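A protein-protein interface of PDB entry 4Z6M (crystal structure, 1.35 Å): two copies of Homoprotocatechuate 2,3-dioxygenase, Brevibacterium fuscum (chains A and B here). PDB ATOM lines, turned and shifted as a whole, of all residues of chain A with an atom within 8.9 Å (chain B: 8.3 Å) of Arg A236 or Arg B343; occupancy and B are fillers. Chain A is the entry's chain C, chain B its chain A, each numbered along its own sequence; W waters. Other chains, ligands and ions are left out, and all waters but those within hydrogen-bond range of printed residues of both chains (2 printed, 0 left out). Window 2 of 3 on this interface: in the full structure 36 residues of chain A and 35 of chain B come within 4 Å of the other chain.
Water W1 lies within hydrogen-bond range of the side-chain hydroxyl of Ser A238 (2.8 Å), the side-chain hydroxyl of Thr B342 (2.8 Å) and the side-chain amide nitrogen of Asn B290 (3.0 Å). Water W2 lies within hydrogen-bond range of the side-chain carboxylate of Asp A239 (3.1 Å) and the guanidinium group of Arg B343 (3.3 Å).
The side-chain carboxylate (OD1) of Asp B289 lies within salt-bridge range of the guanidinium group (NH1) of Arg A236, 2.8 Å away. The side-chain amide nitrogen (NE2) of Gln B291 sits close to the guanidinium group (NE) of Arg A236, 3.4 Å away. The backbone carbonyl oxygen of Thr B342 is in hydrogen-bond range of the guanidinium group of Arg A236 (2.9 Å). NH1 of Arg B343 lies within salt-bridge range of OD1 of Asp A239, at 2.9 Å. NE1 of Trp B295 lies within hydrogen-bond range of O of Asp A230, at 3.0 Å. NE2 of Gln B291 sits at hydrogen-bond distance from O of Gly A233 (2.9 Å). OG of Ser A238 lies within hydrogen-bond range of OE1 of Gln B291 (2.6 Å). O of Arg A236 sits at hydrogen-bond distance from NH1 of Arg B343, at 2.8 Å.
No position is printed for both chains.
Among the printed residues, pairs that only touch across the chains: Ala A234 with Trp B295 (3.4 Å), Gly A233 with Trp B295 (3.4 Å), Asp A239 with Gly B349 (3.5 Å), Asp A239 with Thr B342 (3.6 Å), Ser A238 with Thr B342 (3.6 Å), Arg A236 with Trp B285 (3.8 Å), Ser A238 with Trp B295 (3.9 Å) and Ile A237 with Arg B343 (3.98 Å).
Of chain B, only Trp B285, Asp B289, Gln B291, Thr B342 and Arg B343 come within 4 Å of Arg A236. No residue of chain A comes within 4 Å of Ala B344. Of the printed residues of chain B, Ser A238 touches Gln B291, Trp B295 and Thr B342. Printed residues of chain A within 4 Å of Gln B291: Gly A233, Arg A236 and Ser A238. The nearest printed residue of chain B that does not touch Asp A230 is Gln B291 (6.8 Å).
Printed residues of chain A that touch a printed residue of chain B: Asp A230, Gly A233, Ala A234, Arg A236, Ile A237, Ser A238 and Asp A239. Of the 23 printed residues of chain B, 7 touch a printed residue of chain A. Among the printed residues, Asp or Glu carboxylates within 4 Å of a Lys or Arg side-chain nitrogen of the other chain: Arg A236 with Asp B289 and Asp A239 with Arg B343.
The guanidinium group (NE) of Arg B343 is in salt-bridge range of the side-chain carboxylate (OD2) of Asp B346, at 2.8 Å. The backbone NH (N) of Ile A237 lies within hydrogen-bond range of the backbone carbonyl oxygen (O) of Met A232, at 2.9 Å. O of Asp B289 is in hydrogen-bond range of NH1 of Arg B292 (2.9 Å). The guanidinium group of Arg B343 lies within salt-bridge range of the side-chain carboxylate of Asp B348, at 3.4 Å. The side-chain carboxylate (OD1) of Asp B289 lies within hydrogen-bond range of the backbone NH (N) of Gln B291 (2.9 Å). The side-chain hydroxyl (OG1) of Thr B342 sits at hydrogen-bond distance from the backbone carbonyl oxygen (O) of Gly B349 (2.7 Å).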
ATOM      1  N   CYS A 229       4.011  21.735 -20.763  1.00  0.00           N
ATOM      2  CA  CYS A 229       2.582  21.556 -20.479  1.00  0.00           C
ATOM      3  C   CYS A 229       1.975  22.807 -19.857  1.00  0.00           C
ATOM      4  O   CYS A 229       0.891  23.251 -20.265  1.00  0.00           O
ATOM      5  CB  CYS A 229       2.385  20.377 -19.510  1.00  0.00           C
ATOM      6  SG  CYS A 229       2.910  18.784 -20.126  1.00  0.00           S
ATOM      7  N   ASP A 230       2.647  23.340 -18.842  1.00  0.00           N
ATOM      8  CA  ASP A 230       2.130  24.515 -18.137  1.00  0.00           C
ATOM      9  C   ASP A 230       1.979  25.696 -19.075  1.00  0.00           C
ATOM     10  O   ASP A 230       0.995  26.453 -19.013  1.00  0.00           O
ATOM     11  CB  ASP A 230       3.097  24.882 -17.015  1.00  0.00           C
ATOM     12  CG  ASP A 230       3.077  23.909 -15.842  1.00  0.00           C
ATOM     13  OD1 ASP A 230       2.032  23.253 -15.608  1.00  0.00           O
ATOM     14  OD2 ASP A 230       4.101  23.890 -15.106  1.00  0.00           O
ATOM     15  N   LYS A 231       2.965  25.867 -19.953  1.00  0.00           N
ATOM     16  CA  LYS A 231       2.941  26.962 -20.931  1.00  0.00           C
ATOM     17  C   LYS A 231       1.791  26.809 -21.934  1.00  0.00           C
ATOM     18  O   LYS A 231       1.112  27.760 -22.276  1.00  0.00           O
ATOM     19  CB  LYS A 231       4.283  27.038 -21.675  1.00  0.00           C
ATOM     20  CG  LYS A 231       4.381  28.224 -22.616  1.00  0.00           C
ATOM     21  CD  LYS A 231       5.771  28.396 -23.212  1.00  0.00           C
ATOM     22  CE  LYS A 231       5.890  29.629 -24.082  1.00  0.00           C
ATOM     23  NZ  LYS A 231       7.264  29.736 -24.667  1.00  0.00           N
ATOM     24  N   MET A 232       1.584  25.584 -22.415  1.00  0.00           N
ATOM     25  CA  MET A 232       0.465  25.312 -23.312  1.00  0.00           C
ATOM     26  C   MET A 232      -0.884  25.567 -22.631  1.00  0.00           C
ATOM     27  O   MET A 232      -1.793  26.101 -23.258  1.00  0.00           O
ATOM     28  CB  MET A 232       0.597  23.904 -23.880  1.00  0.00           C
ATOM     29  CG  MET A 232       1.794  23.820 -24.794  1.00  0.00           C
ATOM     30  SD  MET A 232       2.074  22.223 -25.550  1.00  0.00           S
ATOM     31  CE  MET A 232       0.708  22.153 -26.728  1.00  0.00           C
ATOM     32  N   GLY A 233      -0.987  25.271 -21.343  1.00  0.00           N
ATOM     33  CA  GLY A 233      -2.160  25.667 -20.579  1.00  0.00           C
ATOM     34  C   GLY A 233      -2.351  27.189 -20.539  1.00  0.00           C
ATOM     35  O   GLY A 233      -3.451  27.703 -20.770  1.00  0.00           O
ATOM     36  N   ALA A 234      -1.264  27.915 -20.263  1.00  0.00           N
ATOM     37  CA  ALA A 234      -1.348  29.361 -20.184  1.00  0.00           C
ATOM     38  C   ALA A 234      -1.712  29.987 -21.529  1.00  0.00           C
ATOM     39  O   ALA A 234      -2.378  31.016 -21.566  1.00  0.00           O
ATOM     40  CB  ALA A 234      -0.038  29.936 -19.682  1.00  0.00           C
ATOM     41  N   LEU A 235      -1.264  29.386 -22.620  1.00  0.00           N
ATOM     42  CA  LEU A 235      -1.591  29.828 -23.985  1.00  0.00           C
ATOM     43  C   LEU A 235      -2.945  29.300 -24.437  1.00  0.00           C
ATOM     44  O   LEU A 235      -3.371  29.567 -25.556  1.00  0.00           O
ATOM     45  CB  LEU A 235      -0.479  29.399 -24.953  1.00  0.00           C
ATOM     46  CG  LEU A 235       0.868  30.079 -24.727  1.00  0.00           C
ATOM     47  CD1 LEU A 235       1.887  29.424 -25.623  1.00  0.00           C
ATOM     48  CD2 LEU A 235       0.762  31.570 -24.991  1.00  0.00           C
ATOM     49  N   ARG A 236      -3.629  28.564 -23.557  1.00  0.00           N
ATOM     50  CA  ARG A 236      -4.960  28.035 -23.841  1.00  0.00           C
ATOM     51  C   ARG A 236      -4.943  27.176 -25.100  1.00  0.00           C
ATOM     52  O   ARG A 236      -5.866  27.210 -25.913  1.00  0.00           O
ATOM     53  CB  ARG A 236      -5.996  29.164 -23.852  1.00  0.00           C
ATOM     54  CG  ARG A 236      -6.387  29.579 -22.452  1.00  0.00           C
ATOM     55  CD  ARG A 236      -7.434  28.655 -21.876  1.00  0.00           C
ATOM     56  NE  ARG A 236      -7.684  28.953 -20.464  1.00  0.00           N
ATOM     57  CZ  ARG A 236      -8.547  28.262 -19.721  1.00  0.00           C
ATOM     58  NH1 ARG A 236      -9.242  27.291 -20.279  1.00  0.00           N
ATOM     59  NH2 ARG A 236      -8.694  28.515 -18.431  1.00  0.00           N
ATOM     60  N   ILE A 237      -3.888  26.362 -25.212  1.00  0.00           N
ATOM     61  CA  ILE A 237      -3.752  25.367 -26.278  1.00  0.00           C
ATOM     62  C   ILE A 237      -3.507  23.971 -25.692  1.00  0.00           C
ATOM     63  O   ILE A 237      -2.840  23.127 -26.312  1.00  0.00           O
ATOM     64  CB  ILE A 237      -2.691  25.764 -27.342  1.00  0.00           C
ATOM     65  CG1 ILE A 237      -1.317  25.931 -26.703  1.00  0.00           C
ATOM     66  CG2 ILE A 237      -3.172  27.002 -28.093  1.00  0.00           C
ATOM     67  CD1 ILE A 237      -0.180  26.225 -27.656  1.00  0.00           C
ATOM     68  N   SER A 238      -4.134  23.704 -24.543  1.00  0.00           N
ATOM     69  CA  SER A 238      -4.000  22.383 -23.916  1.00  0.00           C
ATOM     70  C   SER A 238      -4.590  21.278 -24.779  1.00  0.00           C
ATOM     71  O   SER A 238      -4.255  20.115 -24.602  1.00  0.00           O
ATOM     72  CB  SER A 238      -4.621  22.337 -22.514  1.00  0.00           C
ATOM     73  OG  SER A 238      -5.962  22.690 -22.514  1.00  0.00           O
ATOM     74  N   ASP A 239      -5.510  21.645 -25.690  1.00  0.00           N
ATOM     75  CA  ASP A 239      -6.031  20.673 -26.657  1.00  0.00           C
ATOM     76  C   ASP A 239      -4.960  20.139 -27.614  1.00  0.00           C
ATOM     77  O   ASP A 239      -5.169  19.123 -28.304  1.00  0.00           O
ATOM     78  CB  ASP A 239      -7.241  21.211 -27.417  1.00  0.00           C
ATOM     79  CG  ASP A 239      -6.979  22.527 -28.151  1.00  0.00           C
ATOM     80  OD1 ASP A 239      -6.167  23.380 -27.701  1.00  0.00           O
ATOM     81  OD2 ASP A 239      -7.682  22.738 -29.170  1.00  0.00           O
ATOM     82  N   ARG A 240      -3.821  20.820 -27.669  1.00  0.00           N
ATOM     83  CA  ARG A 240      -2.704  20.336 -28.486  1.00  0.00           C
ATOM     84  C   ARG A 240      -1.697  19.511 -27.676  1.00  0.00           C
ATOM     85  O   ARG A 240      -0.684  19.071 -28.220  1.00  0.00           O
ATOM     86  CB  ARG A 240      -2.010  21.525 -29.155  1.00  0.00           C
ATOM     87  CG  ARG A 240      -2.931  22.517 -29.880  1.00  0.00           C
ATOM     88  CD  ARG A 240      -3.849  21.833 -30.840  1.00  0.00           C
ATOM     89  NE  ARG A 240      -3.110  21.392 -32.015  1.00  0.00           N
ATOM     90  CZ  ARG A 240      -3.607  20.620 -32.973  1.00  0.00           C
ATOM     91  NH1 ARG A 240      -4.828  20.111 -32.871  1.00  0.00           N
ATOM     92  NH2 ARG A 240      -2.866  20.340 -34.027  1.00  0.00           N
ATOM     93  N   ILE A 241      -1.977  19.291 -26.396  1.00  0.00           N
ATOM     94  CA  ILE A 241      -1.297  18.254 -25.613  1.00  0.00           C
ATOM     95  C   ILE A 241      -2.056  16.965 -25.913  1.00  0.00           C
ATOM     96  O   ILE A 241      -3.196  16.813 -25.499  1.00  0.00           O
ATOM     97  CB  ILE A 241      -1.302  18.554 -24.098  1.00  0.00           C
ATOM     98  CG1 ILE A 241      -0.572  19.856 -23.788  1.00  0.00           C
ATOM     99  CG2 ILE A 241      -0.668  17.409 -23.318  1.00  0.00           C
ATOM    100  CD1 ILE A 241      -0.725  20.340 -22.360  1.00  0.00           C
ATOM    101  N   GLY B 249      -5.655  23.540 -12.213  1.00  0.00           N
ATOM    102  CA  GLY B 249      -6.047  24.910 -12.488  1.00  0.00           C
ATOM    103  C   GLY B 249      -6.273  25.649 -11.185  1.00  0.00           C
ATOM    104  O   GLY B 249      -5.484  26.499 -10.758  1.00  0.00           O
ATOM    105  N   TRP B 285     -13.854  29.618 -11.338  1.00  0.00           N
ATOM    106  CA  TRP B 285     -13.762  28.918 -12.619  1.00  0.00           C
ATOM    107  C   TRP B 285     -15.127  28.425 -13.046  1.00  0.00           C
ATOM    108  O   TRP B 285     -15.940  28.038 -12.198  1.00  0.00           O
ATOM    109  CB  TRP B 285     -12.860  27.708 -12.487  1.00  0.00           C
ATOM    110  CG  TRP B 285     -11.446  28.005 -12.084  1.00  0.00           C
ATOM    111  CD1 TRP B 285     -11.013  28.416 -10.856  1.00  0.00           C
ATOM    112  CD2 TRP B 285     -10.271  27.941 -12.915  1.00  0.00           C
ATOM    113  NE1 TRP B 285      -9.639  28.574 -10.848  1.00  0.00           N
ATOM    114  CE2 TRP B 285      -9.163  28.299 -12.101  1.00  0.00           C
ATOM    115  CE3 TRP B 285     -10.040  27.587 -14.250  1.00  0.00           C
ATOM    116  CZ2 TRP B 285      -7.863  28.318 -12.581  1.00  0.00           C
ATOM    117  CZ3 TRP B 285      -8.723  27.618 -14.723  1.00  0.00           C
ATOM    118  CH2 TRP B 285      -7.671  27.961 -13.877  1.00  0.00           C
ATOM    119  N   ASN B 286     -15.355  28.369 -14.354  1.00  0.00           N
ATOM    120  CA  ASN B 286     -16.565  27.732 -14.869  1.00  0.00           C
ATOM    121  C   ASN B 286     -16.389  26.227 -14.866  1.00  0.00           C
ATOM    122  O   ASN B 286     -15.328  25.722 -15.253  1.00  0.00           O
ATOM    123  CB  ASN B 286     -16.849  28.205 -16.285  1.00  0.00           C
ATOM    124  CG  ASN B 286     -18.204  27.759 -16.768  1.00  0.00           C
ATOM    125  OD1 ASN B 286     -18.325  26.712 -17.410  1.00  0.00           O
ATOM    126  ND2 ASN B 286     -19.228  28.554 -16.487  1.00  0.00           N
ATOM    127  N   HIS B 288     -17.349  24.041 -16.854  1.00  0.00           N
ATOM    128  CA  HIS B 288     -17.103  23.474 -18.172  1.00  0.00           C
ATOM    129  C   HIS B 288     -15.721  23.801 -18.717  1.00  0.00           C
ATOM    130  O   HIS B 288     -15.369  23.330 -19.796  1.00  0.00           O
ATOM    131  CB  HIS B 288     -18.163  23.909 -19.171  1.00  0.00           C
ATOM    132  CG  HIS B 288     -19.552  23.593 -18.729  1.00  0.00           C
ATOM    133  ND1 HIS B 288     -20.133  22.358 -18.892  1.00  0.00           N
ATOM    134  CD2 HIS B 288     -20.467  24.367 -18.093  1.00  0.00           C
ATOM    135  CE1 HIS B 288     -21.352  22.385 -18.376  1.00  0.00           C
ATOM    136  NE2 HIS B 288     -21.576  23.582 -17.876  1.00  0.00           N
ATOM    137  N   ASP B 289     -14.909  24.541 -17.966  1.00  0.00           N
ATOM    138  CA  ASP B 289     -13.541  24.883 -18.399  1.00  0.00           C
ATOM    139  C   ASP B 289     -12.636  23.670 -18.166  1.00  0.00           C
ATOM    140  O   ASP B 289     -12.399  23.275 -17.017  1.00  0.00           O
ATOM    141  CB  ASP B 289     -13.078  26.085 -17.570  1.00  0.00           C
ATOM    142  CG  ASP B 289     -11.693  26.593 -17.947  1.00  0.00           C
ATOM    143  OD1 ASP B 289     -10.902  25.818 -18.516  1.00  0.00           O
ATOM    144  OD2 ASP B 289     -11.416  27.763 -17.628  1.00  0.00           O
ATOM    145  N   ASN B 290     -12.192  23.046 -19.248  1.00  0.00           N
ATOM    146  CA  ASN B 290     -11.415  21.831 -19.163  1.00  0.00           C
ATOM    147  C   ASN B 290     -10.002  22.034 -18.652  1.00  0.00           C
ATOM    148  O   ASN B 290      -9.294  21.057 -18.534  1.00  0.00           O
ATOM    149  CB  ASN B 290     -11.361  21.138 -20.529  1.00  0.00           C
ATOM    150  CG  ASN B 290     -10.852  19.716 -20.441  1.00  0.00           C
ATOM    151  OD1 ASN B 290     -11.384  18.887 -19.691  1.00  0.00           O
ATOM    152  ND2 ASN B 290      -9.811  19.415 -21.214  1.00  0.00           N
ATOM    153  N   GLN B 291      -9.609  23.256 -18.300  1.00  0.00           N
ATOM    154  CA  GLN B 291      -8.341  23.490 -17.605  1.00  0.00           C
ATOM    155  C   GLN B 291      -8.481  23.756 -16.105  1.00  0.00           C
ATOM    156  O   GLN B 291      -7.483  24.031 -15.438  1.00  0.00           O
ATOM    157  CB  GLN B 291      -7.529  24.613 -18.279  1.00  0.00           C
ATOM    158  CG  GLN B 291      -7.170  24.311 -19.724  1.00  0.00           C
ATOM    159  CD  GLN B 291      -6.199  25.275 -20.418  1.00  0.00           C
ATOM    160  OE1 GLN B 291      -5.936  25.125 -21.605  1.00  0.00           O
ATOM    161  NE2 GLN B 291      -5.716  26.274 -19.719  1.00  0.00           N
ATOM    162  N   ARG B 292      -9.696  23.636 -15.563  1.00  0.00           N
ATOM    163  CA  ARG B 292      -9.910  24.062 -14.183  1.00  0.00           C
ATOM    164  C   ARG B 292      -9.341  23.049 -13.181  1.00  0.00           C
ATOM    165  O   ARG B 292      -8.885  23.455 -12.126  1.00  0.00           O
ATOM    166  CB  ARG B 292     -11.384  24.304 -13.902  1.00  0.00           C
ATOM    167  CG  ARG B 292     -12.185  23.009 -13.712  1.00  0.00           C
ATOM    168  CD  ARG B 292     -13.695  23.111 -13.932  1.00  0.00           C
ATOM    169  NE  ARG B 292     -14.290  21.801 -13.701  1.00  0.00           N
ATOM    170  CZ  ARG B 292     -14.199  20.806 -14.568  1.00  0.00           C
ATOM    171  NH1 ARG B 292     -13.651  20.998 -15.757  1.00  0.00           N
ATOM    172  NH2 ARG B 292     -14.685  19.615 -14.258  1.00  0.00           N
ATOM    173  N   ASP B 294      -7.470  19.883 -14.173  1.00  0.00           N
ATOM    174  CA  ASP B 294      -6.164  19.614 -14.769  1.00  0.00           C
ATOM    175  C   ASP B 294      -5.905  20.698 -15.801  1.00  0.00           C
ATOM    176  O   ASP B 294      -6.599  20.784 -16.819  1.00  0.00           O
ATOM    177  CB  ASP B 294      -6.084  18.217 -15.392  1.00  0.00           C
ATOM    178  CG  ASP B 294      -4.690  17.873 -15.761  1.00  0.00           C
ATOM    179  OD1 ASP B 294      -3.915  17.476 -14.842  1.00  0.00           O
ATOM    180  OD2 ASP B 294      -4.321  18.066 -16.928  1.00  0.00           O
ATOM    181  N   TRP B 295      -4.884  21.504 -15.528  1.00  0.00           N
ATOM    182  CA  TRP B 295      -4.536  22.654 -16.360  1.00  0.00           C
ATOM    183  C   TRP B 295      -4.128  22.243 -17.773  1.00  0.00           C
ATOM    184  O   TRP B 295      -4.228  23.031 -18.719  1.00  0.00           O
ATOM    185  CB  TRP B 295      -3.370  23.359 -15.666  1.00  0.00           C
ATOM    186  CG  TRP B 295      -2.798  24.583 -16.290  1.00  0.00           C
ATOM    187  CD1 TRP B 295      -1.505  24.772 -16.655  1.00  0.00           C
ATOM    188  CD2 TRP B 295      -3.459  25.853 -16.463  1.00  0.00           C
ATOM    189  NE1 TRP B 295      -1.304  26.061 -17.090  1.00  0.00           N
ATOM    190  CE2 TRP B 295      -2.500  26.742 -17.005  1.00  0.00           C
ATOM    191  CE3 TRP B 295      -4.771  26.307 -16.278  1.00  0.00           C
ATOM    192  CZ2 TRP B 295      -2.804  28.070 -17.288  1.00  0.00           C
ATOM    193  CZ3 TRP B 295      -5.073  27.646 -16.604  1.00  0.00           C
ATOM    194  CH2 TRP B 295      -4.087  28.491 -17.106  1.00  0.00           C
ATOM    195  N   PHE B 339     -20.400  18.606 -21.307  1.00  0.00           N
ATOM    196  CA  PHE B 339     -19.670  19.490 -22.194  1.00  0.00           C
ATOM    197  C   PHE B 339     -18.479  20.059 -21.454  1.00  0.00           C
ATOM    198  O   PHE B 339     -18.583  20.438 -20.288  1.00  0.00           O
ATOM    199  CB  PHE B 339     -20.572  20.636 -22.655  1.00  0.00           C
ATOM    200  CG  PHE B 339     -19.881  21.630 -23.525  1.00  0.00           C
ATOM    201  CD1 PHE B 339     -19.646  21.362 -24.865  1.00  0.00           C
ATOM    202  CD2 PHE B 339     -19.471  22.846 -23.002  1.00  0.00           C
ATOM    203  CE1 PHE B 339     -18.996  22.302 -25.657  1.00  0.00           C
ATOM    204  CE2 PHE B 339     -18.820  23.780 -23.792  1.00  0.00           C
ATOM    205  CZ  PHE B 339     -18.587  23.498 -25.115  1.00  0.00           C
ATOM    206  N   SER B 340     -17.349  20.161 -22.144  1.00  0.00           N
ATOM    207  CA  SER B 340     -16.262  21.024 -21.693  1.00  0.00           C
ATOM    208  C   SER B 340     -15.571  21.718 -22.848  1.00  0.00           C
ATOM    209  O   SER B 340     -15.660  21.279 -23.999  1.00  0.00           O
ATOM    210  CB  SER B 340     -15.244  20.249 -20.839  1.00  0.00           C
ATOM    211  OG  SER B 340     -14.408  19.411 -21.618  1.00  0.00           O
ATOM    212  N   PHE B 341     -14.875  22.807 -22.533  1.00  0.00           N
ATOM    213  CA  PHE B 341     -14.167  23.601 -23.533  1.00  0.00           C
ATOM    214  C   PHE B 341     -12.711  23.792 -23.155  1.00  0.00           C
ATOM    215  O   PHE B 341     -12.345  23.740 -21.980  1.00  0.00           O
ATOM    216  CB  PHE B 341     -14.850  24.955 -23.774  1.00  0.00           C
ATOM    217  CG  PHE B 341     -14.899  25.861 -22.563  1.00  0.00           C
ATOM    218  CD1 PHE B 341     -13.802  26.602 -22.199  1.00  0.00           C
ATOM    219  CD2 PHE B 341     -16.039  25.958 -21.803  1.00  0.00           C
ATOM    220  CE1 PHE B 341     -13.823  27.418 -21.081  1.00  0.00           C
ATOM    221  CE2 PHE B 341     -16.074  26.769 -20.693  1.00  0.00           C
ATOM    222  CZ  PHE B 341     -14.976  27.518 -20.340  1.00  0.00           C
ATOM    223  N   THR B 342     -11.901  24.074 -24.169  1.00  0.00           N
ATOM    224  CA  THR B 342     -10.521  24.524 -23.966  1.00  0.00           C
ATOM    225  C   THR B 342     -10.460  26.050 -23.937  1.00  0.00           C
ATOM    226  O   THR B 342      -9.870  26.640 -23.048  1.00  0.00           O
ATOM    227  CB  THR B 342      -9.583  23.967 -25.040  1.00  0.00           C
ATOM    228  OG1 THR B 342      -9.595  22.528 -25.003  1.00  0.00           O
ATOM    229  CG2 THR B 342      -8.154  24.452 -24.803  1.00  0.00           C
ATOM    230  N   ARG B 343     -11.131  26.670 -24.904  1.00  0.00           N
ATOM    231  CA  ARG B 343     -11.261  28.111 -24.962  1.00  0.00           C
ATOM    232  C   ARG B 343     -12.740  28.447 -24.962  1.00  0.00           C
ATOM    233  O   ARG B 343     -13.500  27.924 -25.780  1.00  0.00           O
ATOM    234  CB  ARG B 343     -10.615  28.653 -26.231  1.00  0.00           C
ATOM    235  CG  ARG B 343      -9.109  28.488 -26.293  1.00  0.00           C
ATOM    236  CD  ARG B 343      -8.560  28.588 -27.711  1.00  0.00           C
ATOM    237  NE  ARG B 343      -8.999  27.488 -28.549  1.00  0.00           N
ATOM    238  CZ  ARG B 343      -8.416  26.299 -28.638  1.00  0.00           C
ATOM    239  NH1 ARG B 343      -7.303  26.036 -27.949  1.00  0.00           N
ATOM    240  NH2 ARG B 343      -8.968  25.350 -29.407  1.00  0.00           N
ATOM    241  N   ALA B 344     -13.150  29.349 -24.062  1.00  0.00           N
ATOM    242  CA  ALA B 344     -14.555  29.704 -23.961  1.00  0.00           C
ATOM    243  C   ALA B 344     -15.043  30.238 -25.285  1.00  0.00           C
ATOM    244  O   ALA B 344     -14.398  31.062 -25.919  1.00  0.00           O
ATOM    245  CB  ALA B 344     -14.780  30.726 -22.850  1.00  0.00           C
ATOM    246  N   GLY B 345     -16.179  29.721 -25.726  1.00  0.00           N
ATOM    247  CA  GLY B 345     -16.785  30.195 -26.956  1.00  0.00           C
ATOM    248  C   GLY B 345     -16.254  29.559 -28.223  1.00  0.00           C
ATOM    249  O   GLY B 345     -16.749  29.851 -29.307  1.00  0.00           O
ATOM    250  N   ASP B 346     -15.254  28.682 -28.106  1.00  0.00           N
ATOM    251  CA  ASP B 346     -14.602  28.069 -29.274  1.00  0.00           C
ATOM    252  C   ASP B 346     -15.012  26.599 -29.349  1.00  0.00           C
ATOM    253  O   ASP B 346     -14.769  25.841 -28.427  1.00  0.00           O
ATOM    254  CB  ASP B 346     -13.080  28.207 -29.161  1.00  0.00           C
ATOM    255  CG  ASP B 346     -12.318  27.775 -30.422  1.00  0.00           C
ATOM    256  OD1 ASP B 346     -12.951  27.358 -31.414  1.00  0.00           O
ATOM    257  OD2 ASP B 346     -11.059  27.867 -30.414  1.00  0.00           O
ATOM    258  N   GLU B 347     -15.668  26.218 -30.432  1.00  0.00           N
ATOM    259  CA  GLU B 347     -16.029  24.831 -30.669  1.00  0.00           C
ATOM    260  C   GLU B 347     -14.795  23.914 -30.826  1.00  0.00           C
ATOM    261  O   GLU B 347     -14.801  22.757 -30.407  1.00  0.00           O
ATOM    262  CB  GLU B 347     -16.924  24.762 -31.923  1.00  0.00           C
ATOM    263  CG  GLU B 347     -17.489  23.395 -32.204  1.00  0.00           C
ATOM    264  CD  GLU B 347     -18.489  22.958 -31.157  1.00  0.00           C
ATOM    265  OE1 GLU B 347     -19.255  23.810 -30.639  1.00  0.00           O
ATOM    266  OE2 GLU B 347     -18.534  21.749 -30.878  1.00  0.00           O
ATOM    267  N   ASP B 348     -13.740  24.460 -31.405  1.00  0.00           N
ATOM    268  CA  ASP B 348     -12.501  23.728 -31.564  1.00  0.00           C
ATOM    269  C   ASP B 348     -11.843  23.468 -30.203  1.00  0.00           C
ATOM    270  O   ASP B 348     -11.670  24.393 -29.427  1.00  0.00           O
ATOM    271  CB  ASP B 348     -11.579  24.545 -32.463  1.00  0.00           C
ATOM    272  CG  ASP B 348     -10.334  23.811 -32.816  1.00  0.00           C
ATOM    273  OD1 ASP B 348     -10.450  22.640 -33.223  1.00  0.00           O
ATOM    274  OD2 ASP B 348      -9.250  24.402 -32.697  1.00  0.00           O
ATOM    275  N   GLY B 349     -11.498  22.216 -29.902  1.00  0.00           N
ATOM    276  CA  GLY B 349     -11.030  21.863 -28.560  1.00  0.00           C
ATOM    277  C   GLY B 349     -12.106  21.700 -27.495  1.00  0.00           C
ATOM    278  O   GLY B 349     -11.810  21.687 -26.305  1.00  0.00           O
ATOM    279  N   SER B 350     -13.357  21.574 -27.918  1.00  0.00           N
ATOM    280  CA  SER B 350     -14.446  21.291 -26.995  1.00  0.00           C
ATOM    281  C   SER B 350     -14.849  19.833 -27.110  1.00  0.00           C
ATOM    282  O   SER B 350     -14.539  19.151 -28.111  1.00  0.00           O
ATOM    283  CB  SER B 350     -15.648  22.208 -27.258  1.00  0.00           C
ATOM    284  OG  SER B 350     -16.304  21.876 -28.458  1.00  0.00           O
ATOM    285  N   TYR B 351     -15.553  19.376 -26.087  1.00  0.00           N
ATOM    286  CA  TYR B 351     -15.881  17.959 -25.898  1.00  0.00           C
ATOM    287  C   TYR B 351     -17.354  17.866 -25.566  1.00  0.00           C
ATOM    288  O   TYR B 351     -17.816  18.516 -24.646  1.00  0.00           O
ATOM    289  CB  TYR B 351     -15.003  17.338 -24.777  1.00  0.00           C
ATOM    290  CG  TYR B 351     -13.530  17.536 -25.040  1.00  0.00           C
ATOM    291  CD1 TYR B 351     -12.880  16.810 -26.042  1.00  0.00           C
ATOM    292  CD2 TYR B 351     -12.806  18.484 -24.353  1.00  0.00           C
ATOM    293  CE1 TYR B 351     -11.549  17.007 -26.316  1.00  0.00           C
ATOM    294  CE2 TYR B 351     -11.476  18.709 -24.631  1.00  0.00           C
ATOM    295  CZ  TYR B 351     -10.849  17.970 -25.606  1.00  0.00           C
ATOM    296  OH  TYR B 351      -9.519  18.188 -25.878  1.00  0.00           O
HETATM  297  O   HOH W   1      -8.264  21.233 -22.959  1.00  0.00           O
HETATM  298  O   HOH W   2      -5.794  24.733 -30.614  1.00  0.00           O
